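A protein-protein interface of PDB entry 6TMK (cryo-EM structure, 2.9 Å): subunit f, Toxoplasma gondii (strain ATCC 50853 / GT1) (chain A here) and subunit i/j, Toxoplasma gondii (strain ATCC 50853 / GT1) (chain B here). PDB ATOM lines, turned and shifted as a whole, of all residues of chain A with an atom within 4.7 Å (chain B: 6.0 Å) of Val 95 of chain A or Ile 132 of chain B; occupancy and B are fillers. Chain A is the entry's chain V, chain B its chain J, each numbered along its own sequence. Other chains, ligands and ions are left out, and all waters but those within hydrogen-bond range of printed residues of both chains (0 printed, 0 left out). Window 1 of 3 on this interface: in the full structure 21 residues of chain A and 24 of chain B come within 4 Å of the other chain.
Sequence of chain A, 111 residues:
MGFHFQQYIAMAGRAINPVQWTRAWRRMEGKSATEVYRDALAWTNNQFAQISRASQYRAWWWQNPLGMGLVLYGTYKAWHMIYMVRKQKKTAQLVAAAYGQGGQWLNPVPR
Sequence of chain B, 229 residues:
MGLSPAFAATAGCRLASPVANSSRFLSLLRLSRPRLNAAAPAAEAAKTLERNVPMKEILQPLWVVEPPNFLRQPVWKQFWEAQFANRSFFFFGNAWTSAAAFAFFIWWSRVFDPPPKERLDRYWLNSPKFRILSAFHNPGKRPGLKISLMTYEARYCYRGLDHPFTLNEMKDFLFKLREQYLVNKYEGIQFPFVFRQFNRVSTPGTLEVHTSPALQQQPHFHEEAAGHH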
ATOM      1  N   THR A  91     -12.842   0.070  -3.514  1.00  0.00           N
ATOM      2  CA  THR A  91     -12.338  -1.290  -3.652  1.00  0.00           C
ATOM      3  C   THR A  91     -10.832  -1.296  -3.868  1.00  0.00           C
ATOM      4  O   THR A  91     -10.131  -2.185  -3.377  1.00  0.00           O
ATOM      5  CB  THR A  91     -13.058  -1.997  -4.798  1.00  0.00           C
ATOM      6  OG1 THR A  91     -14.466  -1.787  -4.677  1.00  0.00           O
ATOM      7  CG2 THR A  91     -12.767  -3.469  -4.791  1.00  0.00           C
ATOM      8  N   ALA A  92     -10.318  -0.304  -4.588  1.00  0.00           N
ATOM      9  CA  ALA A  92      -8.885  -0.206  -4.813  1.00  0.00           C
ATOM     10  C   ALA A  92      -8.156   0.009  -3.499  1.00  0.00           C
ATOM     11  O   ALA A  92      -7.154  -0.655  -3.216  1.00  0.00           O
ATOM     12  CB  ALA A  92      -8.593   0.922  -5.796  1.00  0.00           C
ATOM     13  N   GLN A  93      -8.644   0.942  -2.685  1.00  0.00           N
ATOM     14  CA  GLN A  93      -8.005   1.199  -1.399  1.00  0.00           C
ATOM     15  C   GLN A  93      -8.105  -0.019  -0.489  1.00  0.00           C
ATOM     16  O   GLN A  93      -7.161  -0.345   0.241  1.00  0.00           O
ATOM     17  CB  GLN A  93      -8.615   2.427  -0.745  1.00  0.00           C
ATOM     18  CG  GLN A  93      -8.364   3.685  -1.497  1.00  0.00           C
ATOM     19  CD  GLN A  93      -8.733   4.915  -0.723  1.00  0.00           C
ATOM     20  OE1 GLN A  93      -7.950   5.428   0.072  1.00  0.00           O
ATOM     21  NE2 GLN A  93      -9.933   5.406  -0.956  1.00  0.00           N
ATOM     22  N   LEU A  94      -9.239  -0.713  -0.534  1.00  0.00           N
ATOM     23  CA  LEU A  94      -9.419  -1.928   0.248  1.00  0.00           C
ATOM     24  C   LEU A  94      -8.394  -2.986  -0.133  1.00  0.00           C
ATOM     25  O   LEU A  94      -7.728  -3.571   0.731  1.00  0.00           O
ATOM     26  CB  LEU A  94     -10.825  -2.452   0.005  1.00  0.00           C
ATOM     27  CG  LEU A  94     -11.327  -3.704   0.708  1.00  0.00           C
ATOM     28  CD1 LEU A  94     -11.445  -3.484   2.180  1.00  0.00           C
ATOM     29  CD2 LEU A  94     -12.622  -4.113   0.104  1.00  0.00           C
ATOM     30  N   VAL A  95      -8.273  -3.262  -1.430  1.00  0.00           N
ATOM     31  CA  VAL A  95      -7.347  -4.285  -1.889  1.00  0.00           C
ATOM     32  C   VAL A  95      -5.914  -3.880  -1.583  1.00  0.00           C
ATOM     33  O   VAL A  95      -5.082  -4.717  -1.224  1.00  0.00           O
ATOM     34  CB  VAL A  95      -7.558  -4.547  -3.390  1.00  0.00           C
ATOM     35  CG1 VAL A  95      -6.475  -5.430  -3.931  1.00  0.00           C
ATOM     36  CG2 VAL A  95      -8.908  -5.163  -3.633  1.00  0.00           C
ATOM     37  N   ALA A  96      -5.601  -2.593  -1.708  1.00  0.00           N
ATOM     38  CA  ALA A  96      -4.240  -2.157  -1.447  1.00  0.00           C
ATOM     39  C   ALA A  96      -3.889  -2.256   0.030  1.00  0.00           C
ATOM     40  O   ALA A  96      -2.730  -2.508   0.372  1.00  0.00           O
ATOM     41  CB  ALA A  96      -4.042  -0.739  -1.961  1.00  0.00           C
ATOM     42  N   ALA A  97      -4.865  -2.070   0.916  1.00  0.00           N
ATOM     43  CA  ALA A  97      -4.609  -2.245   2.337  1.00  0.00           C
ATOM     44  C   ALA A  97      -4.561  -3.711   2.754  1.00  0.00           C
ATOM     45  O   ALA A  97      -3.859  -4.049   3.711  1.00  0.00           O
ATOM     46  CB  ALA A  97      -5.661  -1.502   3.151  1.00  0.00           C
ATOM     47  N   ALA A  98      -5.288  -4.588   2.063  1.00  0.00           N
ATOM     48  CA  ALA A  98      -5.383  -5.991   2.449  1.00  0.00           C
ATOM     49  C   ALA A  98      -4.305  -6.874   1.839  1.00  0.00           C
ATOM     50  O   ALA A  98      -3.812  -7.789   2.503  1.00  0.00           O
ATOM     51  CB  ALA A  98      -6.752  -6.549   2.068  1.00  0.00           C
ATOM     52  N   TYR A  99      -3.932  -6.623   0.591  1.00  0.00           N
ATOM     53  CA  TYR A  99      -2.981  -7.452  -0.131  1.00  0.00           C
ATOM     54  C   TYR A  99      -1.876  -6.670  -0.802  1.00  0.00           C
ATOM     55  O   TYR A  99      -0.834  -7.259  -1.109  1.00  0.00           O
ATOM     56  CB  TYR A  99      -3.688  -8.274  -1.216  1.00  0.00           C
ATOM     57  CG  TYR A  99      -4.917  -9.020  -0.793  1.00  0.00           C
ATOM     58  CD1 TYR A  99      -4.824 -10.244  -0.176  1.00  0.00           C
ATOM     59  CD2 TYR A  99      -6.174  -8.515  -1.044  1.00  0.00           C
ATOM     60  CE1 TYR A  99      -5.941 -10.929   0.200  1.00  0.00           C
ATOM     61  CE2 TYR A  99      -7.291  -9.195  -0.673  1.00  0.00           C
ATOM     62  CZ  TYR A  99      -7.175 -10.405  -0.056  1.00  0.00           C
ATOM     63  OH  TYR A  99      -8.301 -11.091   0.316  1.00  0.00           O
ATOM     64  N   GLY A 100      -2.070  -5.394  -1.067  1.00  0.00           N
ATOM     65  CA  GLY A 100      -1.222  -4.632  -1.950  1.00  0.00           C
ATOM     66  C   GLY A 100      -1.895  -4.372  -3.284  1.00  0.00           C
ATOM     67  O   GLY A 100      -2.845  -5.048  -3.683  1.00  0.00           O
ATOM     68  N   GLY A 102      -2.931  -4.541  -6.820  1.00  0.00           N
ATOM     69  CA  GLY A 102      -2.953  -5.675  -7.711  1.00  0.00           C
ATOM     70  C   GLY A 102      -3.077  -7.007  -7.017  1.00  0.00           C
ATOM     71  O   GLY A 102      -2.875  -8.041  -7.662  1.00  0.00           O
ATOM     72  N   GLY A 103      -3.410  -7.017  -5.726  1.00  0.00           N
ATOM     73  CA  GLY A 103      -3.449  -8.244  -4.963  1.00  0.00           C
ATOM     74  C   GLY A 103      -4.505  -9.229  -5.408  1.00  0.00           C
ATOM     75  O   GLY A 103      -4.364 -10.427  -5.149  1.00  0.00           O
ATOM     76  N   GLN A 104      -5.562  -8.757  -6.062  1.00  0.00           N
ATOM     77  CA  GLN A 104      -6.629  -9.651  -6.475  1.00  0.00           C
ATOM     78  C   GLN A 104      -6.286 -10.381  -7.762  1.00  0.00           C
ATOM     79  O   GLN A 104      -6.933 -11.380  -8.084  1.00  0.00           O
ATOM     80  CB  GLN A 104      -7.952  -8.892  -6.611  1.00  0.00           C
ATOM     81  CG  GLN A 104      -8.109  -7.984  -7.811  1.00  0.00           C
ATOM     82  CD  GLN A 104      -7.387  -6.674  -7.652  1.00  0.00           C
ATOM     83  OE1 GLN A 104      -6.412  -6.573  -6.921  1.00  0.00           O
ATOM     84  NE2 GLN A 104      -7.891  -5.649  -8.305  1.00  0.00           N
ATOM     85  N   SER B 127      -8.889 -16.491  -6.496  1.00  0.00           N
ATOM     86  CA  SER B 127      -9.841 -15.793  -7.336  1.00  0.00           C
ATOM     87  C   SER B 127      -9.985 -14.344  -6.898  1.00  0.00           C
ATOM     88  O   SER B 127      -9.942 -14.052  -5.697  1.00  0.00           O
ATOM     89  CB  SER B 127     -11.208 -16.477  -7.296  1.00  0.00           C
ATOM     90  OG  SER B 127     -12.158 -15.793  -8.070  1.00  0.00           O
ATOM     91  N   PRO B 128     -10.151 -13.418  -7.842  1.00  0.00           N
ATOM     92  CA  PRO B 128     -10.324 -12.021  -7.436  1.00  0.00           C
ATOM     93  C   PRO B 128     -11.599 -11.780  -6.658  1.00  0.00           C
ATOM     94  O   PRO B 128     -11.592 -10.990  -5.709  1.00  0.00           O
ATOM     95  CB  PRO B 128     -10.313 -11.273  -8.775  1.00  0.00           C
ATOM     96  CG  PRO B 128     -10.673 -12.279  -9.777  1.00  0.00           C
ATOM     97  CD  PRO B 128     -10.121 -13.560  -9.303  1.00  0.00           C
ATOM     98  N   LYS B 129     -12.697 -12.436  -7.026  1.00  0.00           N
ATOM     99  CA  LYS B 129     -13.927 -12.306  -6.255  1.00  0.00           C
ATOM    100  C   LYS B 129     -13.713 -12.748  -4.815  1.00  0.00           C
ATOM    101  O   LYS B 129     -14.091 -12.047  -3.871  1.00  0.00           O
ATOM    102  CB  LYS B 129     -15.039 -13.106  -6.923  1.00  0.00           C
ATOM    103  CG  LYS B 129     -16.392 -12.954  -6.296  1.00  0.00           C
ATOM    104  CD  LYS B 129     -17.453 -13.539  -7.173  1.00  0.00           C
ATOM    105  CE  LYS B 129     -18.737 -13.738  -6.421  1.00  0.00           C
ATOM    106  NZ  LYS B 129     -19.340 -12.461  -6.008  1.00  0.00           N
ATOM    107  N   PHE B 130     -13.103 -13.920  -4.632  1.00  0.00           N
ATOM    108  CA  PHE B 130     -12.848 -14.433  -3.295  1.00  0.00           C
ATOM    109  C   PHE B 130     -11.965 -13.486  -2.499  1.00  0.00           C
ATOM    110  O   PHE B 130     -12.248 -13.184  -1.334  1.00  0.00           O
ATOM    111  CB  PHE B 130     -12.213 -15.816  -3.398  1.00  0.00           C
ATOM    112  CG  PHE B 130     -11.643 -16.320  -2.123  1.00  0.00           C
ATOM    113  CD1 PHE B 130     -10.283 -16.395  -1.957  1.00  0.00           C
ATOM    114  CD2 PHE B 130     -12.453 -16.728  -1.095  1.00  0.00           C
ATOM    115  CE1 PHE B 130      -9.754 -16.855  -0.801  1.00  0.00           C
ATOM    116  CE2 PHE B 130     -11.917 -17.189   0.065  1.00  0.00           C
ATOM    117  CZ  PHE B 130     -10.567 -17.253   0.213  1.00  0.00           C
ATOM    118  N   ARG B 131     -10.879 -13.014  -3.109  1.00  0.00           N
ATOM    119  CA  ARG B 131      -9.964 -12.142  -2.392  1.00  0.00           C
ATOM    120  C   ARG B 131     -10.629 -10.828  -2.008  1.00  0.00           C
ATOM    121  O   ARG B 131     -10.481 -10.356  -0.873  1.00  0.00           O
ATOM    122  CB  ARG B 131      -8.732 -11.897  -3.251  1.00  0.00           C
ATOM    123  CG  ARG B 131      -7.821 -13.079  -3.355  1.00  0.00           C
ATOM    124  CD  ARG B 131      -6.877 -12.912  -4.495  1.00  0.00           C
ATOM    125  NE  ARG B 131      -5.865 -13.952  -4.566  1.00  0.00           N
ATOM    126  CZ  ARG B 131      -5.125 -14.180  -5.641  1.00  0.00           C
ATOM    127  NH1 ARG B 131      -5.295 -13.455  -6.726  1.00  0.00           N
ATOM    128  NH2 ARG B 131      -4.215 -15.132  -5.634  1.00  0.00           N
ATOM    129  N   ILE B 132     -11.373 -10.227  -2.936  1.00  0.00           N
ATOM    130  CA  ILE B 132     -12.031  -8.960  -2.647  1.00  0.00           C
ATOM    131  C   ILE B 132     -13.071  -9.134  -1.550  1.00  0.00           C
ATOM    132  O   ILE B 132     -13.188  -8.294  -0.656  1.00  0.00           O
ATOM    133  CB  ILE B 132     -12.633  -8.362  -3.931  1.00  0.00           C
ATOM    134  CG1 ILE B 132     -11.520  -7.838  -4.826  1.00  0.00           C
ATOM    135  CG2 ILE B 132     -13.580  -7.252  -3.607  1.00  0.00           C
ATOM    136  CD1 ILE B 132     -11.905  -7.652  -6.253  1.00  0.00           C
ATOM    137  N   LEU B 133     -13.852 -10.216  -1.607  1.00  0.00           N
ATOM    138  CA  LEU B 133     -14.868 -10.447  -0.585  1.00  0.00           C
ATOM    139  C   LEU B 133     -14.251 -10.692   0.781  1.00  0.00           C
ATOM    140  O   LEU B 133     -14.765 -10.207   1.796  1.00  0.00           O
ATOM    141  CB  LEU B 133     -15.767 -11.613  -0.974  1.00  0.00           C
ATOM    142  CG  LEU B 133     -17.086 -11.273  -1.667  1.00  0.00           C
ATOM    143  CD1 LEU B 133     -16.922 -10.753  -3.054  1.00  0.00           C
ATOM    144  CD2 LEU B 133     -17.917 -12.513  -1.692  1.00  0.00           C
ATOM    145  N   SER B 134     -13.153 -11.443   0.834  1.00  0.00           N
ATOM    146  CA  SER B 134     -12.484 -11.670   2.105  1.00  0.00           C
ATOM    147  C   SER B 134     -11.989 -10.354   2.686  1.00  0.00           C
ATOM    148  O   SER B 134     -12.200 -10.062   3.869  1.00  0.00           O
ATOM    149  CB  SER B 134     -11.334 -12.655   1.914  1.00  0.00           C
ATOM    150  OG  SER B 134     -11.769 -13.829   1.269  1.00  0.00           O
ATOM    151  N   ALA B 135     -11.342  -9.536   1.857  1.00  0.00           N
ATOM    152  CA  ALA B 135     -10.853  -8.248   2.325  1.00  0.00           C
ATOM    153  C   ALA B 135     -11.997  -7.339   2.759  1.00  0.00           C
ATOM    154  O   ALA B 135     -11.868  -6.592   3.734  1.00  0.00           O
ATOM    155  CB  ALA B 135     -10.027  -7.589   1.227  1.00  0.00           C
ATOM    156  N   PHE B 136     -13.127  -7.399   2.056  1.00  0.00           N
ATOM    157  CA  PHE B 136     -14.261  -6.537   2.369  1.00  0.00           C
ATOM    158  C   PHE B 136     -14.914  -6.929   3.685  1.00  0.00           C
ATOM    159  O   PHE B 136     -15.225  -6.068   4.514  1.00  0.00           O
ATOM    160  CB  PHE B 136     -15.280  -6.580   1.231  1.00  0.00           C
ATOM    161  CG  PHE B 136     -16.472  -5.713   1.458  1.00  0.00           C
ATOM    162  CD1 PHE B 136     -16.423  -4.360   1.198  1.00  0.00           C
ATOM    163  CD2 PHE B 136     -17.643  -6.247   1.946  1.00  0.00           C
ATOM    164  CE1 PHE B 136     -17.509  -3.572   1.420  1.00  0.00           C
ATOM    165  CE2 PHE B 136     -18.724  -5.458   2.169  1.00  0.00           C
ATOM    166  CZ  PHE B 136     -18.661  -4.116   1.906  1.00  0.00           C
ATOM    167  N   HIS B 137     -15.149  -8.219   3.889  1.00  0.00           N
ATOM    168  CA  HIS B 137     -15.811  -8.679   5.099  1.00  0.00           C
ATOM    169  C   HIS B 137     -14.856  -8.863   6.267  1.00  0.00           C
ATOM    170  O   HIS B 137     -15.307  -9.218   7.359  1.00  0.00           O
ATOM    171  CB  HIS B 137     -16.576  -9.969   4.820  1.00  0.00           C
ATOM    172  CG  HIS B 137     -17.763  -9.773   3.936  1.00  0.00           C
ATOM    173  ND1 HIS B 137     -18.917  -9.159   4.369  1.00  0.00           N
ATOM    174  CD2 HIS B 137     -17.974 -10.095   2.640  1.00  0.00           C
ATOM    175  CE1 HIS B 137     -19.788  -9.115   3.379  1.00  0.00           C
ATOM    176  NE2 HIS B 137     -19.240  -9.677   2.319  1.00  0.00           N
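The side-chain hydroxyl (OH) of Tyr 99 of chain A is in hydrogen-bond range of the backbone carbonyl oxygen (O) of Arg 131 of chain B (2.6 Å). O of Gln 104 of chain A sits at hydrogen-bond distance from NH1 of Arg 131 of chain B (3.0 Å).
Of the 11 printed residues of chain B, 6 touch a printed residue of chain A.
O of Phe 130 of chain B lies within hydrogen-bond range of OG of Ser 134 of chain B (2.7 Å). N of Gly 100 of chain A sits at hydrogen-bond distance from O of Val 95 of chain A.
Val 95 of chain A touches one residue of chain B. Ile 132 of chain B touches just one residue of chain A: Val 95 (3.9 Å). Of the printed residues of chain A, Pro 128 of chain B touches Gln 104. Printed residues of chain A within 4 Å of Arg 131 of chain B: Tyr 99 (2.6 Å), Gly 103 (3.5 Å) and Gln 104 (3.0 Å). Of the printed residues of chain A, Phe 136 of chain B touches Leu 94 (3.7 Å). Of the printed residues of chain B, Tyr 99 of chain A touches Arg 131 (2.6 Å), Ser 134 (3.8 Å) and Ala 135 (3.7 Å). Printed residues of chain B within 4 Å of Ala 98 of chain A: Ala 135. Gly 100 of chain A touches none of the printed residues of chain B. Thr 91 of chain A touches none of the printed residues of chain B. The nearest residue of chain A that does not touch Ile 132 of chain B is Thr 91 of chain A (4.05 Å).
Among the printed residues, pairs that only touch across the chains: Gln 104 of chain A with Pro 128 of chain B, Leu 94 of chain A with Ala 135 of chain B, Ala 98 of chain A with Ala 135 of chain B, Gly 103 of chain A with Arg 131 of chain B, Tyr 99 of chain A with Ala 135 of chain B, Leu 94 of chain A with Phe 136 of chain B, Tyr 99 of chain A with Ser 134 of chain B and Val 95 of chain A with Ile 132 of chain B.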
